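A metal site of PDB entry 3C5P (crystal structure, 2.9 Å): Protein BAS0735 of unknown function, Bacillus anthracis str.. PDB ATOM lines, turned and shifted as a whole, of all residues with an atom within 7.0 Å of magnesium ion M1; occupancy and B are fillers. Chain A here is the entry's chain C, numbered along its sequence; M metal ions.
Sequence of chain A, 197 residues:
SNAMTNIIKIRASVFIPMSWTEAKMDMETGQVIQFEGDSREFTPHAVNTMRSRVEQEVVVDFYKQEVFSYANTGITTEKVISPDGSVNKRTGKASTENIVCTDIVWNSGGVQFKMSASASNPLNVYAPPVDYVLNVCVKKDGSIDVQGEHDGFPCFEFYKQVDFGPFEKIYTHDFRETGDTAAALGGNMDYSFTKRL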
ATOM      1  N   PRO A 129      -3.695   8.388  14.815  1.00  0.00           N
ATOM      2  CA  PRO A 129      -3.061   8.704  13.549  1.00  0.00           C
ATOM      3  C   PRO A 129      -1.760   9.496  13.715  1.00  0.00           C
ATOM      4  O   PRO A 129      -1.563  10.140  14.749  1.00  0.00           O
ATOM      5  CB  PRO A 129      -4.130   9.523  12.832  1.00  0.00           C
ATOM      6  CG  PRO A 129      -4.907  10.153  13.920  1.00  0.00           C
ATOM      7  CD  PRO A 129      -4.886   9.220  15.068  1.00  0.00           C
ATOM      8  N   ASP A 131       0.389  12.636  12.658  1.00  0.00           N
ATOM      9  CA  ASP A 131      -0.063  13.924  12.197  1.00  0.00           C
ATOM     10  C   ASP A 131       1.119  14.828  11.994  1.00  0.00           C
ATOM     11  O   ASP A 131       2.070  14.772  12.780  1.00  0.00           O
ATOM     12  CB  ASP A 131      -0.921  14.608  13.263  1.00  0.00           C
ATOM     13  CG  ASP A 131      -2.273  13.983  13.414  1.00  0.00           C
ATOM     14  OD1 ASP A 131      -3.066  14.022  12.444  1.00  0.00           O
ATOM     15  OD2 ASP A 131      -2.576  13.480  14.523  1.00  0.00           O
ATOM     16  N   HIS A 150       4.642  18.348  14.584  1.00  0.00           N
ATOM     17  CA  HIS A 150       4.398  16.916  14.330  1.00  0.00           C
ATOM     18  C   HIS A 150       4.310  16.086  15.617  1.00  0.00           C
ATOM     19  O   HIS A 150       4.790  16.549  16.674  1.00  0.00           O
ATOM     20  CB  HIS A 150       5.484  16.362  13.429  1.00  0.00           C
ATOM     21  CG  HIS A 150       6.861  16.575  13.967  1.00  0.00           C
ATOM     22  ND1 HIS A 150       7.514  15.615  14.711  1.00  0.00           N
ATOM     23  CD2 HIS A 150       7.706  17.625  13.872  1.00  0.00           C
ATOM     24  CE1 HIS A 150       8.707  16.073  15.046  1.00  0.00           C
ATOM     25  NE2 HIS A 150       8.851  17.286  14.540  1.00  0.00           N
ATOM     26  N   ASP A 151       3.673  14.913  15.536  1.00  0.00           N
ATOM     27  CA  ASP A 151       3.701  13.911  16.616  1.00  0.00           C
ATOM     28  C   ASP A 151       5.154  13.471  16.846  1.00  0.00           C
ATOM     29  O   ASP A 151       5.997  13.582  15.956  1.00  0.00           O
ATOM     30  CB  ASP A 151       2.859  12.676  16.244  1.00  0.00           C
ATOM     31  CG  ASP A 151       1.330  12.919  16.312  1.00  0.00           C
ATOM     32  OD1 ASP A 151       0.755  13.677  17.135  1.00  0.00           O
ATOM     33  OD2 ASP A 151       0.632  12.258  15.528  1.00  0.00           O
ATOM     34  N   GLY A 152       5.474  12.982  18.050  1.00  0.00           N
ATOM     35  CA  GLY A 152       6.865  12.585  18.342  1.00  0.00           C
ATOM     36  C   GLY A 152       7.320  11.241  17.796  1.00  0.00           C
ATOM     37  O   GLY A 152       8.382  10.733  18.189  1.00  0.00           O
ATOM     38  N   PHE A 153       6.536  10.657  16.892  1.00  0.00           N
ATOM     39  CA  PHE A 153       6.826   9.336  16.350  1.00  0.00           C
ATOM     40  C   PHE A 153       6.054   9.168  15.024  1.00  0.00           C
ATOM     41  O   PHE A 153       4.951   9.676  14.912  1.00  0.00           O
ATOM     42  CB  PHE A 153       6.365   8.276  17.359  1.00  0.00           C
ATOM     43  CG  PHE A 153       6.503   6.866  16.862  1.00  0.00           C
ATOM     44  CD1 PHE A 153       7.693   6.137  17.091  1.00  0.00           C
ATOM     45  CD2 PHE A 153       5.448   6.259  16.158  1.00  0.00           C
ATOM     46  CE1 PHE A 153       7.844   4.815  16.624  1.00  0.00           C
ATOM     47  CE2 PHE A 153       5.586   4.935  15.679  1.00  0.00           C
ATOM     48  CZ  PHE A 153       6.783   4.215  15.916  1.00  0.00           C
ATOM     49  N   ALA A 183       3.597   5.900  21.449  1.00  0.00           N
ATOM     50  CA  ALA A 183       2.618   6.593  22.279  1.00  0.00           C
ATOM     51  C   ALA A 183       2.463   8.026  21.798  1.00  0.00           C
ATOM     52  O   ALA A 183       1.389   8.627  21.934  1.00  0.00           O
ATOM     53  CB  ALA A 183       3.036   6.565  23.752  1.00  0.00           C
ATOM     54  N   ALA A 184       3.536   8.562  21.218  1.00  0.00           N
ATOM     55  CA  ALA A 184       3.578   9.953  20.809  1.00  0.00           C
ATOM     56  C   ALA A 184       2.645  10.204  19.644  1.00  0.00           C
ATOM     57  O   ALA A 184       2.292  11.341  19.347  1.00  0.00           O
ATOM     58  CB  ALA A 184       4.991  10.363  20.464  1.00  0.00           C
ATOM     59  N   LEU A 185       2.226   9.115  18.990  1.00  0.00           N
ATOM     60  CA  LEU A 185       1.198   9.183  17.970  1.00  0.00           C
ATOM     61  C   LEU A 185      -0.088   9.820  18.473  1.00  0.00           C
ATOM     62  O   LEU A 185      -0.801  10.429  17.679  1.00  0.00           O
ATOM     63  CB  LEU A 185       0.876   7.784  17.474  1.00  0.00           C
ATOM     64  CG  LEU A 185       1.252   7.380  16.046  1.00  0.00           C
ATOM     65  CD1 LEU A 185       2.361   8.231  15.452  1.00  0.00           C
ATOM     66  CD2 LEU A 185       1.634   5.904  16.000  1.00  0.00           C
ATOM     67  N   GLY A 186      -0.365   9.660  19.765  1.00  0.00           N
ATOM     68  CA  GLY A 186      -1.637  10.027  20.333  1.00  0.00           C
ATOM     69  C   GLY A 186      -1.628  11.398  20.972  1.00  0.00           C
ATOM     70  O   GLY A 186      -0.583  12.009  21.135  1.00  0.00           O
ATOM     71  N   GLY A 187      -2.821  11.880  21.334  1.00  0.00           N
ATOM     72  CA  GLY A 187      -2.976  13.161  22.006  1.00  0.00           C
ATOM     73  C   GLY A 187      -2.714  14.267  21.011  1.00  0.00           C
ATOM     74  O   GLY A 187      -3.290  14.283  19.921  1.00  0.00           O
ATOM     75  N   ASN A 188      -1.826  15.182  21.386  1.00  0.00           N
ATOM     76  CA  ASN A 188      -1.540  16.348  20.554  1.00  0.00           C
ATOM     77  C   ASN A 188      -0.305  16.227  19.676  1.00  0.00           C
ATOM     78  O   ASN A 188       0.432  15.244  19.782  1.00  0.00           O
ATOM     79  CB  ASN A 188      -1.405  17.535  21.485  1.00  0.00           C
ATOM     80  CG  ASN A 188      -2.728  18.069  21.886  1.00  0.00           C
ATOM     81  OD1 ASN A 188      -3.688  17.985  21.117  1.00  0.00           O
ATOM     82  ND2 ASN A 188      -2.806  18.611  23.100  1.00  0.00           N
ATOM     83  N   MET A 189      -0.085  17.219  18.815  1.00  0.00           N
ATOM     84  CA  MET A 189       1.200  17.321  18.130  1.00  0.00           C
ATOM     85  C   MET A 189       2.241  17.931  19.061  1.00  0.00           C
ATOM     86  O   MET A 189       2.269  19.136  19.326  1.00  0.00           O
ATOM     87  CB  MET A 189       1.091  18.065  16.826  1.00  0.00           C
ATOM     88  CG  MET A 189       0.639  17.178  15.717  1.00  0.00           C
ATOM     89  SD  MET A 189       0.386  18.208  14.086  1.00  0.00           S
ATOM     90  CE  MET A 189      -1.239  19.270  14.508  1.00  0.00           C
ATOM     91  N   ASP A 190       3.110  17.054  19.540  1.00  0.00           N
ATOM     92  CA  ASP A 190       3.957  17.324  20.666  1.00  0.00           C
ATOM     93  C   ASP A 190       5.326  17.960  20.359  1.00  0.00           C
ATOM     94  O   ASP A 190       6.110  18.142  21.264  1.00  0.00           O
ATOM     95  CB  ASP A 190       4.070  16.047  21.557  1.00  0.00           C
ATOM     96  CG  ASP A 190       4.300  14.700  20.735  1.00  0.00           C
ATOM     97  OD1 ASP A 190       3.518  14.330  19.814  1.00  0.00           O
ATOM     98  OD2 ASP A 190       5.244  13.963  21.084  1.00  0.00           O
HETATM   99 MG    MG M   1       0.906  13.043  19.723  1.00  0.00          MG
HETATM  100 MG    MG M   2      -1.804  11.916  15.919  1.00  0.00          MG
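Magnesium ion M1 is bound by O of Ala 184, O of Asn 188 and O of Gly 186. Slightly farther from magnesium ion M1 lies the side-chain carboxylate (OD1) of Asp 151 (2.7 Å).
The side-chain carboxylate (OD1) of Asp 190 lies within hydrogen-bond range of the backbone NH (N) of Gly 152, at 3.0 Å. The backbone NH (N) of Asp 190 is in hydrogen-bond range of the backbone carbonyl oxygen (O) of His 150.
Merely in contact with magnesium ion M1: Leu 185 and Asp 190. Of the 14 residues printed, 6 come within 4 Å of magnesium ion M1.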
